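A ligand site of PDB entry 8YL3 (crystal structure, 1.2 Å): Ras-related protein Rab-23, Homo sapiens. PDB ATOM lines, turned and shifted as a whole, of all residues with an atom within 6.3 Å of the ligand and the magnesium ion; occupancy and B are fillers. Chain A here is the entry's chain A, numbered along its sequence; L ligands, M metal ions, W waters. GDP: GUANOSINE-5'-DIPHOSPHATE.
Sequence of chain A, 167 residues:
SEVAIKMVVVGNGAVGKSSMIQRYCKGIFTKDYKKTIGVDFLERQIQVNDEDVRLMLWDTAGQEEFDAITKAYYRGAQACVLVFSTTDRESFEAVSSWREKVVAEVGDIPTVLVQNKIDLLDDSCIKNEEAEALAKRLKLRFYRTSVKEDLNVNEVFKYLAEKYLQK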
ATOM      1  N   GLY A  11      16.969  21.088  23.485  1.00  0.00           N
ATOM      2  CA  GLY A  11      15.671  20.437  23.409  1.00  0.00           C
ATOM      3  C   GLY A  11      15.625  19.242  24.341  1.00  0.00           C
ATOM      4  O   GLY A  11      16.630  18.833  24.911  1.00  0.00           O
ATOM      5  N   ASN A  12      14.429  18.676  24.470  1.00  0.00           N
ATOM      6  CA  ASN A  12      14.206  17.573  25.406  1.00  0.00           C
ATOM      7  C   ASN A  12      15.034  16.334  25.019  1.00  0.00           C
ATOM      8  O   ASN A  12      15.551  16.205  23.913  1.00  0.00           O
ATOM      9  CB  ASN A  12      12.724  17.193  25.433  1.00  0.00           C
ATOM     10  CG  ASN A  12      11.924  18.060  26.370  1.00  0.00           C
ATOM     11  OD1 ASN A  12      12.336  19.175  26.720  1.00  0.00           O
ATOM     12  ND2 ASN A  12      10.779  17.554  26.815  1.00  0.00           N
ATOM     13  N   GLY A  13      15.124  15.415  25.974  1.00  0.00           N
ATOM     14  CA  GLY A  13      15.885  14.197  25.742  1.00  0.00           C
ATOM     15  C   GLY A  13      15.326  13.401  24.582  1.00  0.00           C
ATOM     16  O   GLY A  13      14.105  13.320  24.377  1.00  0.00           O
ATOM     17  N   ALA A  14      16.226  12.800  23.815  1.00  0.00           N
ATOM     18  CA  ALA A  14      15.920  11.833  22.764  1.00  0.00           C
ATOM     19  C   ALA A  14      15.293  12.443  21.522  1.00  0.00           C
ATOM     20  O   ALA A  14      14.840  11.696  20.640  1.00  0.00           O
ATOM     21  CB  ALA A  14      15.107  10.626  23.260  1.00  0.00           C
ATOM     22  N   VAL A  15      15.271  13.770  21.400  1.00  0.00           N
ATOM     23  CA  VAL A  15      14.733  14.383  20.190  1.00  0.00           C
ATOM     24  C   VAL A  15      15.674  14.226  18.996  1.00  0.00           C
ATOM     25  O   VAL A  15      15.247  14.420  17.853  1.00  0.00           O
ATOM     26  CB  VAL A  15      14.306  15.853  20.379  1.00  0.00           C
ATOM     27  CG1 VAL A  15      13.289  15.978  21.486  1.00  0.00           C
ATOM     28  CG2 VAL A  15      15.512  16.741  20.664  1.00  0.00           C
ATOM     29  N   GLY A  16      16.932  13.892  19.243  1.00  0.00           N
ATOM     30  CA  GLY A  16      17.912  13.694  18.191  1.00  0.00           C
ATOM     31  C   GLY A  16      19.035  14.712  18.111  1.00  0.00           C
ATOM     32  O   GLY A  16      19.645  14.840  17.048  1.00  0.00           O
ATOM     33  N   LYS A  17      19.343  15.417  19.215  1.00  0.00           N
ATOM     34  CA  LYS A  17      20.354  16.469  19.192  1.00  0.00           C
ATOM     35  C   LYS A  17      21.735  15.918  18.896  1.00  0.00           C
ATOM     36  O   LYS A  17      22.440  16.411  17.997  1.00  0.00           O
ATOM     37  CB  LYS A  17      20.354  17.188  20.546  1.00  0.00           C
ATOM     38  CG  LYS A  17      19.010  17.839  20.903  1.00  0.00           C
ATOM     39  CD  LYS A  17      19.075  18.587  22.238  1.00  0.00           C
ATOM     40  CE  LYS A  17      19.409  17.681  23.412  1.00  0.00           C
ATOM     41  NZ  LYS A  17      18.359  16.641  23.665  1.00  0.00           N
ATOM     42  N   SER A  18      22.154  14.878  19.622  1.00  0.00           N
ATOM     43  CA  SER A  18      23.474  14.291  19.384  1.00  0.00           C
ATOM     44  C   SER A  18      23.569  13.727  17.984  1.00  0.00           C
ATOM     45  O   SER A  18      24.566  13.921  17.286  1.00  0.00           O
ATOM     46  CB  SER A  18      23.762  13.195  20.425  1.00  0.00           C
ATOM     47  OG  SER A  18      23.712  13.711  21.753  1.00  0.00           O
ATOM     48  N   SER A  19      22.502  13.042  17.538  1.00  0.00           N
ATOM     49  CA  SER A  19      22.477  12.500  16.192  1.00  0.00           C
ATOM     50  C   SER A  19      22.591  13.609  15.160  1.00  0.00           C
ATOM     51  O   SER A  19      23.302  13.460  14.157  1.00  0.00           O
ATOM     52  CB  SER A  19      21.166  11.725  15.957  1.00  0.00           C
ATOM     53  OG  SER A  19      21.006  10.640  16.859  1.00  0.00           O
ATOM     54  N   MET A  20      21.899  14.728  15.387  1.00  0.00           N
ATOM     55  CA  MET A  20      21.946  15.819  14.427  1.00  0.00           C
ATOM     56  C   MET A  20      23.360  16.358  14.280  1.00  0.00           C
ATOM     57  O   MET A  20      23.813  16.630  13.158  1.00  0.00           O
ATOM     58  CB  MET A  20      20.997  16.930  14.872  1.00  0.00           C
ATOM     59  CG  MET A  20      20.867  18.074  13.870  1.00  0.00           C
ATOM     60  SD  MET A  20      19.677  19.316  14.412  1.00  0.00           S
ATOM     61  CE  MET A  20      18.157  18.359  14.468  1.00  0.00           C
ATOM     62  N   PHE A  29      24.847   8.312  10.440  1.00  0.00           N
ATOM     63  CA  PHE A  29      23.716   8.069  11.326  1.00  0.00           C
ATOM     64  C   PHE A  29      23.695   6.586  11.657  1.00  0.00           C
ATOM     65  O   PHE A  29      23.588   5.759  10.747  1.00  0.00           O
ATOM     66  CB  PHE A  29      22.397   8.480  10.685  1.00  0.00           C
ATOM     67  CG  PHE A  29      21.192   8.187  11.533  1.00  0.00           C
ATOM     68  CD1 PHE A  29      20.769   9.092  12.490  1.00  0.00           C
ATOM     69  CD2 PHE A  29      20.480   7.011  11.383  1.00  0.00           C
ATOM     70  CE1 PHE A  29      19.661   8.826  13.279  1.00  0.00           C
ATOM     71  CE2 PHE A  29      19.379   6.737  12.175  1.00  0.00           C
ATOM     72  CZ  PHE A  29      18.962   7.643  13.120  1.00  0.00           C
ATOM     73  N   THR A  30      23.779   6.248  12.929  1.00  0.00           N
ATOM     74  CA  THR A  30      23.666   4.864  13.378  1.00  0.00           C
ATOM     75  C   THR A  30      22.313   4.641  14.033  1.00  0.00           C
ATOM     76  O   THR A  30      21.594   5.574  14.376  1.00  0.00           O
ATOM     77  CB  THR A  30      24.815   4.505  14.329  1.00  0.00           C
ATOM     78  OG1 THR A  30      24.733   5.310  15.504  1.00  0.00           O
ATOM     79  CG2 THR A  30      26.159   4.736  13.647  1.00  0.00           C
ATOM     80  N   LYS A  31      21.960   3.361  14.210  1.00  0.00           N
ATOM     81  CA  LYS A  31      20.643   2.997  14.722  1.00  0.00           C
ATOM     82  C   LYS A  31      20.609   2.800  16.246  1.00  0.00           C
ATOM     83  O   LYS A  31      19.693   2.148  16.751  1.00  0.00           O
ATOM     84  CB  LYS A  31      20.109   1.756  14.002  1.00  0.00           C
ATOM     85  CG  LYS A  31      20.020   1.913  12.501  1.00  0.00           C
ATOM     86  CD  LYS A  31      19.566   0.628  11.834  1.00  0.00           C
ATOM     87  CE  LYS A  31      19.594   0.751  10.324  1.00  0.00           C
ATOM     88  NZ  LYS A  31      19.164  -0.507   9.660  1.00  0.00           N
ATOM     89  N   ASP A  32      21.578   3.349  16.969  1.00  0.00           N
ATOM     90  CA  ASP A  32      21.622   3.215  18.426  1.00  0.00           C
ATOM     91  C   ASP A  32      20.492   3.997  19.086  1.00  0.00           C
ATOM     92  O   ASP A  32      20.051   5.023  18.567  1.00  0.00           O
ATOM     93  CB  ASP A  32      22.965   3.732  18.938  1.00  0.00           C
ATOM     94  CG  ASP A  32      24.152   3.038  18.271  1.00  0.00           C
ATOM     95  OD1 ASP A  32      24.271   1.806  18.410  1.00  0.00           O
ATOM     96  OD2 ASP A  32      24.947   3.721  17.595  1.00  0.00           O
ATOM     97  N   TYR A  33      20.032   3.527  20.256  1.00  0.00           N
ATOM     98  CA  TYR A  33      18.940   4.212  20.950  1.00  0.00           C
ATOM     99  C   TYR A  33      19.347   5.573  21.500  1.00  0.00           C
ATOM    100  O   TYR A  33      18.479   6.418  21.733  1.00  0.00           O
ATOM    101  CB  TYR A  33      18.389   3.340  22.089  1.00  0.00           C
ATOM    102  CG  TYR A  33      19.088   3.563  23.405  1.00  0.00           C
ATOM    103  CD1 TYR A  33      20.321   2.964  23.663  1.00  0.00           C
ATOM    104  CD2 TYR A  33      18.522   4.366  24.394  1.00  0.00           C
ATOM    105  CE1 TYR A  33      20.971   3.171  24.864  1.00  0.00           C
ATOM    106  CE2 TYR A  33      19.173   4.578  25.603  1.00  0.00           C
ATOM    107  CZ  TYR A  33      20.396   3.981  25.826  1.00  0.00           C
ATOM    108  OH  TYR A  33      21.051   4.175  27.022  1.00  0.00           O
ATOM    109  N   LYS A  34      20.641   5.792  21.734  1.00  0.00           N
ATOM    110  CA  LYS A  34      21.122   7.054  22.266  1.00  0.00           C
ATOM    111  C   LYS A  34      22.505   7.296  21.679  1.00  0.00           C
ATOM    112  O   LYS A  34      23.343   6.392  21.636  1.00  0.00           O
ATOM    113  CB  LYS A  34      21.197   7.019  23.797  1.00  0.00           C
ATOM    114  CG  LYS A  34      21.695   8.318  24.398  1.00  0.00           C
ATOM    115  CD  LYS A  34      21.673   8.253  25.917  1.00  0.00           C
ATOM    116  CE  LYS A  34      22.254   9.515  26.517  1.00  0.00           C
ATOM    117  NZ  LYS A  34      21.495  10.721  26.076  1.00  0.00           N
ATOM    118  N   LYS A  35      22.739   8.517  21.233  1.00  0.00           N
ATOM    119  CA  LYS A  35      24.022   8.891  20.660  1.00  0.00           C
ATOM    120  C   LYS A  35      24.802   9.697  21.679  1.00  0.00           C
ATOM    121  O   LYS A  35      24.220  10.458  22.468  1.00  0.00           O
ATOM    122  CB  LYS A  35      23.822   9.681  19.371  1.00  0.00           C
ATOM    123  CG  LYS A  35      23.583   8.798  18.132  1.00  0.00           C
ATOM    124  CD  LYS A  35      22.334   7.924  18.245  1.00  0.00           C
ATOM    125  CE  LYS A  35      22.120   7.061  17.024  1.00  0.00           C
ATOM    126  NZ  LYS A  35      21.769   7.893  15.830  1.00  0.00           N
ATOM    127  N   THR A  36      26.115   9.530  21.683  1.00  0.00           N
ATOM    128  CA  THR A  36      26.971  10.237  22.622  1.00  0.00           C
ATOM    129  C   THR A  36      28.129  10.892  21.892  1.00  0.00           C
ATOM    130  O   THR A  36      28.626  10.375  20.880  1.00  0.00           O
ATOM    131  CB  THR A  36      27.532   9.317  23.719  1.00  0.00           C
ATOM    132  OG1 THR A  36      28.276   8.264  23.111  1.00  0.00           O
ATOM    133  CG2 THR A  36      26.413   8.731  24.566  1.00  0.00           C
ATOM    134  N   ASP A  59      27.090  19.904  22.187  1.00  0.00           N
ATOM    135  CA  ASP A  59      26.060  18.930  22.502  1.00  0.00           C
ATOM    136  C   ASP A  59      25.857  18.865  24.002  1.00  0.00           C
ATOM    137  O   ASP A  59      26.832  18.764  24.760  1.00  0.00           O
ATOM    138  CB  ASP A  59      26.492  17.545  22.011  1.00  0.00           C
ATOM    139  CG  ASP A  59      25.353  16.559  21.974  1.00  0.00           C
ATOM    140  OD1 ASP A  59      24.174  16.966  21.800  1.00  0.00           O
ATOM    141  OD2 ASP A  59      25.648  15.362  22.122  1.00  0.00           O
ATOM    142  N   THR A  60      24.600  18.921  24.429  1.00  0.00           N
ATOM    143  CA  THR A  60      24.262  18.795  25.846  1.00  0.00           C
ATOM    144  C   THR A  60      24.474  17.363  26.312  1.00  0.00           C
ATOM    145  O   THR A  60      24.271  16.397  25.571  1.00  0.00           O
ATOM    146  CB  THR A  60      22.808  19.163  26.084  1.00  0.00           C
ATOM    147  OG1 THR A  60      21.954  18.194  25.478  1.00  0.00           O
ATOM    148  CG2 THR A  60      22.486  20.533  25.509  1.00  0.00           C
ATOM    149  N   ALA A  61      24.884  17.226  27.576  1.00  0.00           N
ATOM    150  CA  ALA A  61      25.009  15.915  28.193  1.00  0.00           C
ATOM    151  C   ALA A  61      23.686  15.411  28.775  1.00  0.00           C
ATOM    152  O   ALA A  61      23.522  14.195  28.927  1.00  0.00           O
ATOM    153  CB  ALA A  61      26.073  15.938  29.290  1.00  0.00           C
ATOM    154  N   ASN A 116      12.387  17.484  14.360  1.00  0.00           N
ATOM    155  CA  ASN A 116      13.152  16.339  13.896  1.00  0.00           C
ATOM    156  C   ASN A 116      12.279  15.078  13.854  1.00  0.00           C
ATOM    157  O   ASN A 116      11.142  15.069  14.329  1.00  0.00           O
ATOM    158  CB  ASN A 116      14.381  16.130  14.793  1.00  0.00           C
ATOM    159  CG  ASN A 116      15.363  15.140  14.213  1.00  0.00           C
ATOM    160  OD1 ASN A 116      15.545  15.063  12.994  1.00  0.00           O
ATOM    161  ND2 ASN A 116      15.998  14.350  15.076  1.00  0.00           N
ATOM    162  N   LYS A 117      12.840  14.025  13.265  1.00  0.00           N
ATOM    163  CA  LYS A 117      12.178  12.723  13.094  1.00  0.00           C
ATOM    164  C   LYS A 117      10.958  12.798  12.188  1.00  0.00           C
ATOM    165  O   LYS A 117       9.998  12.047  12.366  1.00  0.00           O
ATOM    166  CB  LYS A 117      11.838  12.048  14.432  1.00  0.00           C
ATOM    167  CG  LYS A 117      12.955  12.084  15.474  1.00  0.00           C
ATOM    168  CD  LYS A 117      12.734  11.048  16.572  1.00  0.00           C
ATOM    169  CE  LYS A 117      13.822  11.139  17.632  1.00  0.00           C
ATOM    170  NZ  LYS A 117      13.635  10.123  18.698  1.00  0.00           N
ATOM    171  N   ILE A 118      10.993  13.700  11.212  1.00  0.00           N
ATOM    172  CA  ILE A 118       9.851  13.860  10.308  1.00  0.00           C
ATOM    173  C   ILE A 118       9.632  12.620   9.451  1.00  0.00           C
ATOM    174  O   ILE A 118       8.556  12.462   8.848  1.00  0.00           O
ATOM    175  CB  ILE A 118      10.018  15.158   9.481  1.00  0.00           C
ATOM    176  CG1 ILE A 118       8.665  15.697   9.016  1.00  0.00           C
ATOM    177  CG2 ILE A 118      10.963  14.954   8.306  1.00  0.00           C
ATOM    178  CD1 ILE A 118       7.811  16.247  10.138  1.00  0.00           C
ATOM    179  N   ASP A 119      10.618  11.720   9.381  1.00  0.00           N
ATOM    180  CA  ASP A 119      10.415  10.440   8.718  1.00  0.00           C
ATOM    181  C   ASP A 119       9.414   9.555   9.455  1.00  0.00           C
ATOM    182  O   ASP A 119       8.919   8.586   8.863  1.00  0.00           O
ATOM    183  CB  ASP A 119      11.753   9.710   8.585  1.00  0.00           C
ATOM    184  CG  ASP A 119      12.450   9.515   9.926  1.00  0.00           C
ATOM    185  OD1 ASP A 119      12.980  10.516  10.479  1.00  0.00           O
ATOM    186  OD2 ASP A 119      12.452   8.375  10.437  1.00  0.00           O
ATOM    187  N   LEU A 120       9.108   9.858  10.713  1.00  0.00           N
ATOM    188  CA  LEU A 120       8.127   9.127  11.501  1.00  0.00           C
ATOM    189  C   LEU A 120       6.760   9.804  11.467  1.00  0.00           C
ATOM    190  O   LEU A 120       6.013   9.755  12.452  1.00  0.00           O
ATOM    191  CB  LEU A 120       8.623   8.967  12.937  1.00  0.00           C
ATOM    192  CG  LEU A 120       9.997   8.298  13.098  1.00  0.00           C
ATOM    193  CD1 LEU A 120      10.396   8.216  14.558  1.00  0.00           C
ATOM    194  CD2 LEU A 120      10.023   6.932  12.455  1.00  0.00           C
ATOM    195  N   THR A 145      12.653  18.208   9.670  1.00  0.00           N
ATOM    196  CA  THR A 145      13.951  17.605   9.446  1.00  0.00           C
ATOM    197  C   THR A 145      13.898  16.108   9.756  1.00  0.00           C
ATOM    198  O   THR A 145      13.148  15.666  10.639  1.00  0.00           O
ATOM    199  CB  THR A 145      14.948  18.317  10.371  1.00  0.00           C
ATOM    200  OG1 THR A 145      15.091  19.679   9.943  1.00  0.00           O
ATOM    201  CG2 THR A 145      16.308  17.652  10.386  1.00  0.00           C
ATOM    202  N   SER A 146      14.709  15.335   9.046  1.00  0.00           N
ATOM    203  CA  SER A 146      15.012  13.959   9.434  1.00  0.00           C
ATOM    204  C   SER A 146      16.526  13.795   9.451  1.00  0.00           C
ATOM    205  O   SER A 146      17.165  13.775   8.397  1.00  0.00           O
ATOM    206  CB  SER A 146      14.396  12.932   8.487  1.00  0.00           C
ATOM    207  OG  SER A 146      14.823  11.626   8.844  1.00  0.00           O
ATOM    208  N   VAL A 147      17.103  13.695  10.650  1.00  0.00           N
ATOM    209  CA  VAL A 147      18.515  13.343  10.750  1.00  0.00           C
ATOM    210  C   VAL A 147      18.759  11.967  10.150  1.00  0.00           C
ATOM    211  O   VAL A 147      19.774  11.730   9.472  1.00  0.00           O
ATOM    212  CB  VAL A 147      18.974  13.435  12.217  1.00  0.00           C
ATOM    213  CG1 VAL A 147      20.400  12.953  12.365  1.00  0.00           C
ATOM    214  CG2 VAL A 147      18.849  14.877  12.728  1.00  0.00           C
ATOM    215  N   LYS A 148      17.831  11.043  10.378  1.00  0.00           N
ATOM    216  CA  LYS A 148      17.987   9.673   9.886  1.00  0.00           C
ATOM    217  C   LYS A 148      18.082   9.615   8.365  1.00  0.00           C
ATOM    218  O   LYS A 148      18.921   8.888   7.814  1.00  0.00           O
ATOM    219  CB  LYS A 148      16.821   8.825  10.370  1.00  0.00           C
ATOM    220  CG  LYS A 148      16.776   7.431   9.757  1.00  0.00           C
ATOM    221  CD  LYS A 148      15.649   6.590  10.327  1.00  0.00           C
ATOM    222  CE  LYS A 148      15.674   5.169   9.794  1.00  0.00           C
ATOM    223  NZ  LYS A 148      14.525   4.389  10.314  1.00  0.00           N
ATOM    224  N   GLU A 149      17.224  10.360   7.666  1.00  0.00           N
ATOM    225  CA  GLU A 149      17.195  10.342   6.212  1.00  0.00           C
ATOM    226  C   GLU A 149      17.955  11.503   5.585  1.00  0.00           C
ATOM    227  O   GLU A 149      17.930  11.667   4.360  1.00  0.00           O
ATOM    228  CB  GLU A 149      15.739  10.282   5.715  1.00  0.00           C
ATOM    229  CG  GLU A 149      14.981   9.053   6.205  1.00  0.00           C
ATOM    230  CD  GLU A 149      15.602   7.742   5.742  1.00  0.00           C
ATOM    231  OE1 GLU A 149      16.193   7.710   4.644  1.00  0.00           O
ATOM    232  OE2 GLU A 149      15.489   6.731   6.477  1.00  0.00           O
HETATM  233  PB  GDP L   1      19.318  13.443  22.115  1.00  0.00           P
HETATM  234  O1B GDP L   1      20.794  13.756  21.939  1.00  0.00           O
HETATM  235  O2B GDP L   1      18.420  14.603  21.752  1.00  0.00           O
HETATM  236  O3B GDP L   1      18.987  12.848  23.470  1.00  0.00           O
HETATM  237  O3A GDP L   1      18.998  12.298  21.016  1.00  0.00           O
HETATM  238  PA  GDP L   1      19.859  11.172  20.292  1.00  0.00           P
HETATM  239  O1A GDP L   1      20.666  11.797  19.227  1.00  0.00           O
HETATM  240  O2A GDP L   1      20.525  10.364  21.332  1.00  0.00           O
HETATM  241  O5' GDP L   1      18.719  10.349  19.538  1.00  0.00           O
HETATM  242  C5' GDP L   1      17.711   9.622  20.268  1.00  0.00           C
HETATM  243  C4' GDP L   1      17.194   8.533  19.358  1.00  0.00           C
HETATM  244  O4' GDP L   1      16.478   9.126  18.239  1.00  0.00           O
HETATM  245  C3' GDP L   1      18.259   7.641  18.735  1.00  0.00           C
HETATM  246  O3' GDP L   1      17.779   6.302  18.631  1.00  0.00           O
HETATM  247  C2' GDP L   1      18.446   8.250  17.345  1.00  0.00           C
HETATM  248  O2' GDP L   1      19.014   7.395  16.367  1.00  0.00           O
HETATM  249  C1' GDP L   1      16.991   8.605  17.033  1.00  0.00           C
HETATM  250  N9  GDP L   1      16.850   9.611  15.990  1.00  0.00           N
HETATM  251  C8  GDP L   1      17.536  10.795  15.872  1.00  0.00           C
HETATM  252  N7  GDP L   1      17.195  11.496  14.825  1.00  0.00           N
HETATM  253  C5  GDP L   1      16.216  10.725  14.204  1.00  0.00           C
HETATM  254  C6  GDP L   1      15.459  10.952  13.022  1.00  0.00           C
HETATM  255  O6  GDP L   1      15.519  11.934  12.279  1.00  0.00           O
HETATM  256  N1  GDP L   1      14.579   9.928  12.762  1.00  0.00           N
HETATM  257  C2  GDP L   1      14.429   8.797  13.522  1.00  0.00           C
HETATM  258  N2  GDP L   1      13.530   7.893  13.111  1.00  0.00           N
HETATM  259  N3  GDP L   1      15.127   8.566  14.632  1.00  0.00           N
HETATM  260  C4  GDP L   1      16.000   9.561  14.913  1.00  0.00           C
HETATM  261 MG    MG M   1      22.333  13.601  23.308  1.00  0.00          MG
HETATM  262  O   HOH W   1      13.642   7.692  17.035  1.00  0.00           O
HETATM  263  O   HOH W   2      22.470  15.657  23.449  1.00  0.00           O
HETATM  264  O   HOH W   3      13.469   5.123  13.961  1.00  0.00           O
HETATM  265  O   HOH W   4      18.966  10.495  24.738  1.00  0.00           O
HETATM  266  O   HOH W   5      17.749   4.992  15.783  1.00  0.00           O
HETATM  267  O   HOH W   6      23.956  13.329  24.632  1.00  0.00           O
HETATM  268  O   HOH W   7      22.163  11.497  23.169  1.00  0.00           O
HETATM  269  O   HOH W   8      21.062  13.579  24.933  1.00  0.00           O
HETATM  270  O   HOH W   9      17.244   3.192  17.673  1.00  0.00           O
HETATM  271  O   HOH W  10      15.141   5.615  18.047  1.00  0.00           O
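An oxygen (O2B) of the ligand lies within salt-bridge range of the side-chain amino group (NZ) of Lys 17, 2.8 Å away.
The side-chain amide nitrogen (ND2) of Asn 116 is in hydrogen-bond range of a nitrogen (N7) of the ligand.
The backbone NH (N) of Lys 148 is in hydrogen-bond range of an oxygen (O6) of the ligand.
O6 of the ligand sits at hydrogen-bond distance from N of Val 147 (2.9 Å).
O of Tyr 33 is in hydrogen-bond range of O3' of the ligand.
The backbone carbonyl oxygen (O) of Asp 32 is in hydrogen-bond range of an oxygen (O3') of the ligand (2.6 Å).
An oxygen (O1A) of the ligand lies within hydrogen-bond range of the backbone NH (N) of Ser 18, at 3.4 Å.
An oxygen (O2B) of the ligand lies within hydrogen-bond range of the backbone NH of Lys 17, 2.8 Å away.
NZ of Lys 35 sits at hydrogen-bond distance from O2' of the ligand (2.9 Å).
The backbone NH (N) of Ala 14 sits at hydrogen-bond distance from an oxygen (O3B) of the ligand (2.8 Å).
O1A of the ligand lies within hydrogen-bond range of OG of Ser 19, at 2.7 Å.
The side-chain carboxylate of Asp 119 lies within hydrogen-bond range of a nitrogen (N1) of the ligand (2.8 Å).
The backbone NH of Lys 35 lies within hydrogen-bond range of an oxygen (O2A) of the ligand (2.9 Å).
N of Val 15 lies within hydrogen-bond range of O2B of the ligand, 3.3 Å away.
The backbone NH of Ser 19 is in hydrogen-bond range of an oxygen (O1A) of the ligand, 2.8 Å away.
The side-chain amino group (NZ) of Lys 117 lies within hydrogen-bond range of an oxygen (O4') of the ligand, at 3.0 Å.
The backbone NH of Gly 16 is in hydrogen-bond range of an oxygen (O2B) of the ligand.
N of Val 147 is in hydrogen-bond range of OD1 of Asn 116.
OD1 of Asn 116 lies close to O of Thr 145 (3.4 Å).
The side-chain hydroxyl of Ser 19 lies within hydrogen-bond range of the side-chain amino group of Lys 35 (3.0 Å).
NZ of Lys 17 sits at hydrogen-bond distance from O of Asn 12 (2.9 Å).
The backbone NH (N) of Lys 148 lies close to the side-chain hydroxyl (OG) of Ser 146, 3.4 Å away.
N of Glu 149 lies within hydrogen-bond range of OG of Ser 146, 3.0 Å away.
The side-chain amino group (NZ) of Lys 35 sits at hydrogen-bond distance from the backbone carbonyl oxygen (O) of Thr 30 (2.7 Å).
O of Thr 145 sits at hydrogen-bond distance from N of Lys 117 (3.1 Å).
Asn 12 touches the ligand.
Gly 13 touches the ligand (C to O3B, 3.9 Å).
Phe 29 touches the ligand.
Thr 30 touches the ligand (O to O2', 3.7 Å).
Lys 34 touches the ligand.
Leu 120 touches the ligand.
Ser 146 touches the ligand.
Hydrophobic or aromatic side chains that line the ligand: Val 15, Phe 29, Leu 120 and Val 147.
Within 4 Å of the ligand: Asn 12, Gly 13, Ala 14, Val 15, Gly 16, Lys 17, Ser 18, Ser 19, Phe 29, Thr 30, Asp 32, Tyr 33, Lys 34, Lys 35, Asn 116, Lys 117, Asp 119, Leu 120, Ser 146, Val 147 and Lys 148.
The nearest printed residue that does not touch the ligand is Asp 59 (4.7 Å).
Residues that only touch the magnesium ion: Lys 35 and Asp 59.
Three residues have an atom within 4 Å of the magnesium ion: Ser 18, Lys 35 and Asp 59.
The nearest printed residue that does not touch the magnesium ion is Lys 34 (4.1 Å).
The magnesium ion is bound by water W8 (2.1 Å), water W2 (2.1 Å), O1B of the ligand (2.1 Å), OG of Ser 18 (2.1 Å), water W6 (2.1 Å) and water W7 (2.1 Å).
Water W2 bridges the side-chain carboxylate of Asp 59 (2.7 Å) and the backbone carbonyl oxygen of Thr 60 (2.9 Å).
Water W8 lies within hydrogen-bond range of an oxygen (O3B) of the ligand and the side-chain amino group (NZ) of Lys 34.
Water W7 lies within hydrogen-bond range of O of Lys 35 (2.4 Å), O2A of the ligand (2.7 Å) and NZ of Lys 34 (3.1 Å).
Water W4 bridges an oxygen (O3B) of the ligand (2.7 Å) and the side-chain amino group of Lys 34 (2.9 Å).
Water W1 lies within hydrogen-bond range of NZ of Lys 117 (2.9 Å) and N3 of the ligand (3.0 Å).
Water W9 lies within hydrogen-bond range of O of Lys 31 (2.8 Å), O3' of the ligand (3.3 Å) and O of Asp 32 (3.5 Å).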
